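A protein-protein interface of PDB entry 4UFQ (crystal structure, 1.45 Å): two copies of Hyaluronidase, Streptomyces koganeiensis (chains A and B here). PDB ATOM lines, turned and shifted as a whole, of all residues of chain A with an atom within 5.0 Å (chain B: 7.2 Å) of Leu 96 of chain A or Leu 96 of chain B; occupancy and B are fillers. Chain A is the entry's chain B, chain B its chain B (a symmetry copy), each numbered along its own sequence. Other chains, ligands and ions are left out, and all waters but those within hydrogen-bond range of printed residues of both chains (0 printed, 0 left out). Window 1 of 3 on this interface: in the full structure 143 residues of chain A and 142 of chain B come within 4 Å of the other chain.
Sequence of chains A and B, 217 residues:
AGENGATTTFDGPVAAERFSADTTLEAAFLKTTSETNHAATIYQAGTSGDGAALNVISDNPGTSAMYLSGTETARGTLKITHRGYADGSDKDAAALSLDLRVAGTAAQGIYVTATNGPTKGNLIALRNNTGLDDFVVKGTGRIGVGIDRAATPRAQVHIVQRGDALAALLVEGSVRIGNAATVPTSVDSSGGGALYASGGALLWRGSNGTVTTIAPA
N of Tyr 111 of chain A lies within hydrogen-bond range of O of Leu 96 of chain B (2.9 Å). N of Thr 77 of chain B is in hydrogen-bond range of O of Ala 94 of chain A, at 2.9 Å. The backbone NH (N) of Ala 94 of chain A lies within hydrogen-bond range of the backbone carbonyl oxygen (O) of Arg 75 of chain B, at 3.2 Å. The backbone NH of Leu 96 of chain B lies within hydrogen-bond range of the backbone carbonyl oxygen of Gly 109 of chain A (3.0 Å). The backbone NH of Leu 98 of chain B sits at hydrogen-bond distance from the backbone carbonyl oxygen of Tyr 111 of chain A (2.8 Å). The backbone carbonyl oxygen (O) of Gly 109 of chain A sits at hydrogen-bond distance from the backbone NH (N) of Ala 95 of chain B (3.3 Å). The backbone NH (N) of Ser 97 of chain A sits at hydrogen-bond distance from the backbone carbonyl oxygen (O) of Leu 78 of chain B (2.9 Å). O of Ala 95 of chain A sits close to N of Thr 77 of chain B, 3.4 Å away. O of Ala 95 of chain A lies within hydrogen-bond range of N of Leu 78 of chain B (3.1 Å). O of Ser 97 of chain A lies within hydrogen-bond range of N of Ile 80 of chain B, 2.8 Å away.
Among the printed residues, pairs that only touch across the chains: Ala 94 of chain A with Gly 76 of chain B, Ile 80 of chain A with Leu 68 of chain B, Leu 98 of chain A with Ile 80 of chain B, Tyr 111 of chain A with Ser 97 of chain B, Ser 97 of chain A with Lys 79 of chain B, Ile 110 of chain A with Leu 96 of chain B, Leu 96 of chain A with Leu 78 of chain B, Ile 110 of chain A with Ile 110 of chain B, Ile 80 of chain A with Thr 77 of chain B, Ile 80 of chain A with Leu 78 of chain B and Leu 96 of chain A with Leu 96 of chain B.
Printed residues of chain B within 4 Å of Leu 96 of chain A: Leu 78 (3.5 Å) and Leu 96 (3.97 Å). Of chain A, only Leu 96 (3.97 Å), Gly 109 (3.0 Å), Ile 110 (3.4 Å) and Tyr 111 (2.9 Å) come within 4 Å of Leu 96 of chain B. Of the printed residues of chain B, Gly 109 of chain A touches Ala 95 and Leu 96. Of the printed residues of chain A, Ala 95 of chain B touches Gly 109 (3.3 Å). Printed residues of chain A within 4 Å of Gly 76 of chain B: Ala 94. Printed residues of chain B within 4 Å of Ala 95 of chain A: Thr 77 (3.3 Å) and Leu 78 (3.1 Å). Ala 94 of chain B touches none of the printed residues of chain A. Ala 93 of chain B touches none of the printed residues of chain A. The nearest residue of chain B that does not touch Leu 96 of chain A is Ile 80 of chain B (4.3 Å). The nearest residue of chain A that does not touch Leu 96 of chain B is Leu 98 of chain A (4.3 Å).
Hydrophobic or aromatic side chains of chain A that line the printed part of chain B: Ile 80, Leu 96, Leu 98, Ile 110 and Tyr 111. Hydrophobic or aromatic side chains of chain B that line the printed part of chain A: Leu 78, Ile 80, Ala 95, Leu 96 and Ile 110. Among the printed residues, 21 pairs touch across the chains. Among the printed residues, no Asp or Glu carboxylate lies within 4 Å of a Lys or Arg side-chain nitrogen of the other chain.
Leu 96 of chain A touches its own counterpart, Leu 96 of chain B. Ser 97 of chain A touches Ile 80 of chain B, but with the chains exchanged Ile 80 of chain A does not touch Ser 97 of chain B (11.8 Å). Leu 98 of chain A touches Ile 80 of chain B, but with the chains exchanged Ile 80 of chain A does not touch Leu 98 of chain B (9.5 Å). Ile 110 of chain A touches its own counterpart, Ile 110 of chain B. Of the 21 pairs that touch across the chains among the printed residues, 2 have their exchanged pair printed and touching as well.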
ATOM      1  N   ILE A  80      16.807  23.000 -23.916  1.00  0.00           N
ATOM      2  CA  ILE A  80      17.705  21.998 -23.376  1.00  0.00           C
ATOM      3  C   ILE A  80      18.443  21.301 -24.499  1.00  0.00           C
ATOM      4  O   ILE A  80      17.826  20.720 -25.386  1.00  0.00           O
ATOM      5  CB  ILE A  80      16.972  20.934 -22.535  1.00  0.00           C
ATOM      6  CG1 ILE A  80      16.105  21.577 -21.446  1.00  0.00           C
ATOM      7  CG2 ILE A  80      17.984  19.961 -21.928  1.00  0.00           C
ATOM      8  CD1 ILE A  80      15.359  20.574 -20.535  1.00  0.00           C
ATOM      9  N   ALA A  94      19.049  11.165 -21.042  1.00  0.00           N
ATOM     10  CA  ALA A  94      17.869  11.812 -21.570  1.00  0.00           C
ATOM     11  C   ALA A  94      18.077  13.316 -21.503  1.00  0.00           C
ATOM     12  O   ALA A  94      18.945  13.785 -20.769  1.00  0.00           O
ATOM     13  CB  ALA A  94      16.623  11.401 -20.777  1.00  0.00           C
ATOM     14  N   ALA A  95      17.312  14.075 -22.280  1.00  0.00           N
ATOM     15  CA  ALA A  95      17.323  15.528 -22.136  1.00  0.00           C
ATOM     16  C   ALA A  95      16.533  15.959 -20.904  1.00  0.00           C
ATOM     17  O   ALA A  95      16.931  16.897 -20.197  1.00  0.00           O
ATOM     18  CB  ALA A  95      16.777  16.216 -23.381  1.00  0.00           C
ATOM     19  N   LEU A  96      15.418  15.266 -20.659  1.00  0.00           N
ATOM     20  CA  LEU A  96      14.509  15.604 -19.576  1.00  0.00           C
ATOM     21  C   LEU A  96      14.058  14.331 -18.885  1.00  0.00           C
ATOM     22  O   LEU A  96      13.506  13.430 -19.539  1.00  0.00           O
ATOM     23  CB  LEU A  96      13.297  16.362 -20.112  1.00  0.00           C
ATOM     24  CG  LEU A  96      12.272  16.779 -19.057  1.00  0.00           C
ATOM     25  CD1 LEU A  96      12.881  17.784 -18.095  1.00  0.00           C
ATOM     26  CD2 LEU A  96      11.033  17.369 -19.702  1.00  0.00           C
ATOM     27  N   SER A  97      14.279  14.253 -17.574  1.00  0.00           N
ATOM     28  CA  SER A  97      13.861  13.103 -16.785  1.00  0.00           C
ATOM     29  C   SER A  97      13.029  13.528 -15.583  1.00  0.00           C
ATOM     30  O   SER A  97      13.458  14.379 -14.811  1.00  0.00           O
ATOM     31  CB  SER A  97      15.089  12.320 -16.349  1.00  0.00           C
ATOM     32  OG  SER A  97      14.739  11.179 -15.591  1.00  0.00           O
ATOM     33  N   LEU A  98      11.837  12.950 -15.443  1.00  0.00           N
ATOM     34  CA  LEU A  98      10.895  13.290 -14.375  1.00  0.00           C
ATOM     35  C   LEU A  98      10.640  12.067 -13.516  1.00  0.00           C
ATOM     36  O   LEU A  98      10.390  10.982 -14.040  1.00  0.00           O
ATOM     37  CB  LEU A  98       9.555  13.778 -14.948  1.00  0.00           C
ATOM     38  CG  LEU A  98       9.585  14.846 -16.044  1.00  0.00           C
ATOM     39  CD1 LEU A  98       8.159  15.231 -16.414  1.00  0.00           C
ATOM     40  CD2 LEU A  98      10.369  16.072 -15.675  1.00  0.00           C
ATOM     41  N   GLY A 109       2.611  13.990 -14.350  1.00  0.00           N
ATOM     42  CA  GLY A 109       3.909  14.124 -14.989  1.00  0.00           C
ATOM     43  C   GLY A 109       4.064  15.462 -15.700  1.00  0.00           C
ATOM     44  O   GLY A 109       4.724  16.369 -15.198  1.00  0.00           O
ATOM     45  N   ILE A 110       3.446  15.582 -16.872  1.00  0.00           N
ATOM     46  CA  ILE A 110       3.547  16.759 -17.725  1.00  0.00           C
ATOM     47  C   ILE A 110       2.149  17.314 -18.003  1.00  0.00           C
ATOM     48  O   ILE A 110       1.270  16.574 -18.470  1.00  0.00           O
ATOM     49  CB  ILE A 110       4.213  16.385 -19.065  1.00  0.00           C
ATOM     50  CG1 ILE A 110       5.642  15.882 -18.815  1.00  0.00           C
ATOM     51  CG2 ILE A 110       4.209  17.580 -20.042  1.00  0.00           C
ATOM     52  CD1 ILE A 110       6.293  15.220 -20.021  1.00  0.00           C
ATOM     53  N   TYR A 111       1.956  18.607 -17.734  1.00  0.00           N
ATOM     54  CA  TYR A 111       0.666  19.267 -17.908  1.00  0.00           C
ATOM     55  C   TYR A 111       0.870  20.463 -18.808  1.00  0.00           C
ATOM     56  O   TYR A 111       1.745  21.281 -18.541  1.00  0.00           O
ATOM     57  CB  TYR A 111       0.135  19.729 -16.551  1.00  0.00           C
ATOM     58  CG  TYR A 111      -1.323  20.152 -16.552  1.00  0.00           C
ATOM     59  CD1 TYR A 111      -1.705  21.457 -16.852  1.00  0.00           C
ATOM     60  CD2 TYR A 111      -2.315  19.230 -16.255  1.00  0.00           C
ATOM     61  CE1 TYR A 111      -3.053  21.821 -16.856  1.00  0.00           C
ATOM     62  CE2 TYR A 111      -3.651  19.582 -16.259  1.00  0.00           C
ATOM     63  CZ  TYR A 111      -4.017  20.870 -16.560  1.00  0.00           C
ATOM     64  OH  TYR A 111      -5.358  21.192 -16.553  1.00  0.00           O
ATOM     65  N   LEU B  68      19.944  25.376 -21.149  1.00  0.00           N
ATOM     66  CA  LEU B  68      20.565  24.323 -20.358  1.00  0.00           C
ATOM     67  C   LEU B  68      21.284  23.355 -21.292  1.00  0.00           C
ATOM     68  O   LEU B  68      20.689  22.847 -22.237  1.00  0.00           O
ATOM     69  CB  LEU B  68      19.522  23.600 -19.522  1.00  0.00           C
ATOM     70  CG  LEU B  68      20.016  22.407 -18.712  1.00  0.00           C
ATOM     71  CD1 LEU B  68      21.018  22.852 -17.652  1.00  0.00           C
ATOM     72  CD2 LEU B  68      18.868  21.691 -18.047  1.00  0.00           C
ATOM     73  N   ARG B  75      22.213   9.873 -17.362  1.00  0.00           N
ATOM     74  CA  ARG B  75      21.275  10.633 -16.543  1.00  0.00           C
ATOM     75  C   ARG B  75      20.560  11.659 -17.399  1.00  0.00           C
ATOM     76  O   ARG B  75      20.924  11.874 -18.546  1.00  0.00           O
ATOM     77  CB  ARG B  75      22.013  11.346 -15.412  1.00  0.00           C
ATOM     78  CG  ARG B  75      22.748  10.416 -14.464  1.00  0.00           C
ATOM     79  CD  ARG B  75      21.791   9.576 -13.634  1.00  0.00           C
ATOM     80  NE  ARG B  75      22.502   8.721 -12.684  1.00  0.00           N
ATOM     81  CZ  ARG B  75      22.914   7.479 -12.935  1.00  0.00           C
ATOM     82  NH1 ARG B  75      22.689   6.911 -14.113  1.00  0.00           N
ATOM     83  NH2 ARG B  75      23.552   6.796 -11.995  1.00  0.00           N
ATOM     84  N   GLY B  76      19.545  12.299 -16.825  1.00  0.00           N
ATOM     85  CA  GLY B  76      18.830  13.368 -17.504  1.00  0.00           C
ATOM     86  C   GLY B  76      19.592  14.689 -17.429  1.00  0.00           C
ATOM     87  O   GLY B  76      20.228  14.983 -16.410  1.00  0.00           O
ATOM     88  N   THR B  77      19.547  15.483 -18.502  1.00  0.00           N
ATOM     89  CA  THR B  77      20.203  16.800 -18.509  1.00  0.00           C
ATOM     90  C   THR B  77      19.531  17.723 -17.490  1.00  0.00           C
ATOM     91  O   THR B  77      20.204  18.443 -16.736  1.00  0.00           O
ATOM     92  CB  THR B  77      20.208  17.455 -19.927  1.00  0.00           C
ATOM     93  OG1 THR B  77      20.834  16.563 -20.861  1.00  0.00           O
ATOM     94  CG2 THR B  77      20.965  18.777 -19.919  1.00  0.00           C
ATOM     95  N   LEU B  78      18.197  17.715 -17.510  1.00  0.00           N
ATOM     96  CA  LEU B  78      17.391  18.257 -16.426  1.00  0.00           C
ATOM     97  C   LEU B  78      16.652  17.084 -15.773  1.00  0.00           C
ATOM     98  O   LEU B  78      15.927  16.334 -16.457  1.00  0.00           O
ATOM     99  CB  LEU B  78      16.396  19.298 -16.946  1.00  0.00           C
ATOM    100  CG  LEU B  78      15.391  19.816 -15.910  1.00  0.00           C
ATOM    101  CD1 LEU B  78      16.086  20.427 -14.672  1.00  0.00           C
ATOM    102  CD2 LEU B  78      14.451  20.827 -16.527  1.00  0.00           C
ATOM    103  N   LYS B  79      16.858  16.918 -14.468  1.00  0.00           N
ATOM    104  CA  LYS B  79      16.186  15.906 -13.674  1.00  0.00           C
ATOM    105  C   LYS B  79      15.269  16.575 -12.677  1.00  0.00           C
ATOM    106  O   LYS B  79      15.726  17.313 -11.796  1.00  0.00           O
ATOM    107  CB  LYS B  79      17.196  15.016 -12.954  1.00  0.00           C
ATOM    108  CG  LYS B  79      16.595  14.033 -11.949  1.00  0.00           C
ATOM    109  CD  LYS B  79      15.813  12.947 -12.637  1.00  0.00           C
ATOM    110  CE  LYS B  79      15.244  11.959 -11.628  1.00  0.00           C
ATOM    111  NZ  LYS B  79      16.308  11.172 -10.978  1.00  0.00           N
ATOM    112  N   ILE B  80      13.972  16.316 -12.826  1.00  0.00           N
ATOM    113  CA  ILE B  80      12.967  16.878 -11.944  1.00  0.00           C
ATOM    114  C   ILE B  80      12.368  15.791 -11.079  1.00  0.00           C
ATOM    115  O   ILE B  80      11.825  14.814 -11.587  1.00  0.00           O
ATOM    116  CB  ILE B  80      11.827  17.579 -12.711  1.00  0.00           C
ATOM    117  CG1 ILE B  80      12.372  18.618 -13.701  1.00  0.00           C
ATOM    118  CG2 ILE B  80      10.852  18.220 -11.724  1.00  0.00           C
ATOM    119  CD1 ILE B  80      11.289  19.391 -14.489  1.00  0.00           C
ATOM    120  N   HIS B  82       9.521  15.234  -8.102  1.00  0.00           N
ATOM    121  CA  HIS B  82       8.429  15.688  -7.249  1.00  0.00           C
ATOM    122  C   HIS B  82       8.287  14.718  -6.084  1.00  0.00           C
ATOM    123  O   HIS B  82       8.020  13.521  -6.283  1.00  0.00           O
ATOM    124  CB  HIS B  82       7.109  15.800  -8.016  1.00  0.00           C
ATOM    125  CG  HIS B  82       5.963  16.215  -7.152  1.00  0.00           C
ATOM    126  ND1 HIS B  82       5.139  15.300  -6.532  1.00  0.00           N
ATOM    127  CD2 HIS B  82       5.530  17.437  -6.761  1.00  0.00           C
ATOM    128  CE1 HIS B  82       4.236  15.942  -5.813  1.00  0.00           C
ATOM    129  NE2 HIS B  82       4.454  17.242  -5.931  1.00  0.00           N
ATOM    130  N   ALA B  93      -0.997  18.579  -8.386  1.00  0.00           N
ATOM    131  CA  ALA B  93       0.396  18.909  -8.655  1.00  0.00           C
ATOM    132  C   ALA B  93       0.903  18.217  -9.926  1.00  0.00           C
ATOM    133  O   ALA B  93       0.266  17.299 -10.467  1.00  0.00           O
ATOM    134  CB  ALA B  93       1.264  18.520  -7.465  1.00  0.00           C
ATOM    135  N   ALA B  94       2.057  18.669 -10.407  1.00  0.00           N
ATOM    136  CA  ALA B  94       2.698  18.072 -11.557  1.00  0.00           C
ATOM    137  C   ALA B  94       4.201  18.249 -11.414  1.00  0.00           C
ATOM    138  O   ALA B  94       4.650  19.089 -10.637  1.00  0.00           O
ATOM    139  CB  ALA B  94       2.197  18.715 -12.854  1.00  0.00           C
ATOM    140  N   ALA B  95       4.982  17.450 -12.132  1.00  0.00           N
ATOM    141  CA  ALA B  95       6.422  17.682 -12.190  1.00  0.00           C
ATOM    142  C   ALA B  95       6.748  18.857 -13.108  1.00  0.00           C
ATOM    143  O   ALA B  95       7.651  19.654 -12.814  1.00  0.00           O
ATOM    144  CB  ALA B  95       7.170  16.435 -12.644  1.00  0.00           C
ATOM    145  N   LEU B  96       6.004  18.952 -14.213  1.00  0.00           N
ATOM    146  CA  LEU B  96       6.243  19.962 -15.231  1.00  0.00           C
ATOM    147  C   LEU B  96       4.913  20.528 -15.696  1.00  0.00           C
ATOM    148  O   LEU B  96       4.039  19.771 -16.149  1.00  0.00           O
ATOM    149  CB  LEU B  96       6.994  19.359 -16.417  1.00  0.00           C
ATOM    150  CG  LEU B  96       7.308  20.335 -17.551  1.00  0.00           C
ATOM    151  CD1 LEU B  96       8.269  21.409 -17.074  1.00  0.00           C
ATOM    152  CD2 LEU B  96       7.897  19.612 -18.746  1.00  0.00           C
ATOM    153  N   SER B  97       4.759  21.847 -15.595  1.00  0.00           N
ATOM    154  CA  SER B  97       3.548  22.521 -16.040  1.00  0.00           C
ATOM    155  C   SER B  97       3.868  23.662 -16.996  1.00  0.00           C
ATOM    156  O   SER B  97       4.681  24.522 -16.674  1.00  0.00           O
ATOM    157  CB  SER B  97       2.779  23.024 -14.829  1.00  0.00           C
ATOM    158  OG  SER B  97       1.582  23.675 -15.204  1.00  0.00           O
ATOM    159  N   LEU B  98       3.243  23.652 -18.173  1.00  0.00           N
ATOM    160  CA  LEU B  98       3.484  24.644 -19.222  1.00  0.00           C
ATOM    161  C   LEU B  98       2.201  25.400 -19.509  1.00  0.00           C
ATOM    162  O   LEU B  98       1.144  24.789 -19.667  1.00  0.00           O
ATOM    163  CB  LEU B  98       3.963  23.977 -20.521  1.00  0.00           C
ATOM    164  CG  LEU B  98       5.099  22.956 -20.431  1.00  0.00           C
ATOM    165  CD1 LEU B  98       5.461  22.475 -21.830  1.00  0.00           C
ATOM    166  CD2 LEU B  98       6.325  23.471 -19.732  1.00  0.00           C
ATOM    167  N   ILE B 110       5.686  21.592 -26.489  1.00  0.00           N
ATOM    168  CA  ILE B 110       6.918  20.824 -26.355  1.00  0.00           C
ATOM    169  C   ILE B 110       7.444  20.448 -27.741  1.00  0.00           C
ATOM    170  O   ILE B 110       6.706  19.856 -28.544  1.00  0.00           O
ATOM    171  CB  ILE B 110       6.652  19.535 -25.553  1.00  0.00           C
ATOM    172  CG1 ILE B 110       6.182  19.888 -24.135  1.00  0.00           C
ATOM    173  CG2 ILE B 110       7.906  18.635 -25.511  1.00  0.00           C
ATOM    174  CD1 ILE B 110       5.620  18.712 -23.350  1.00  0.00           C
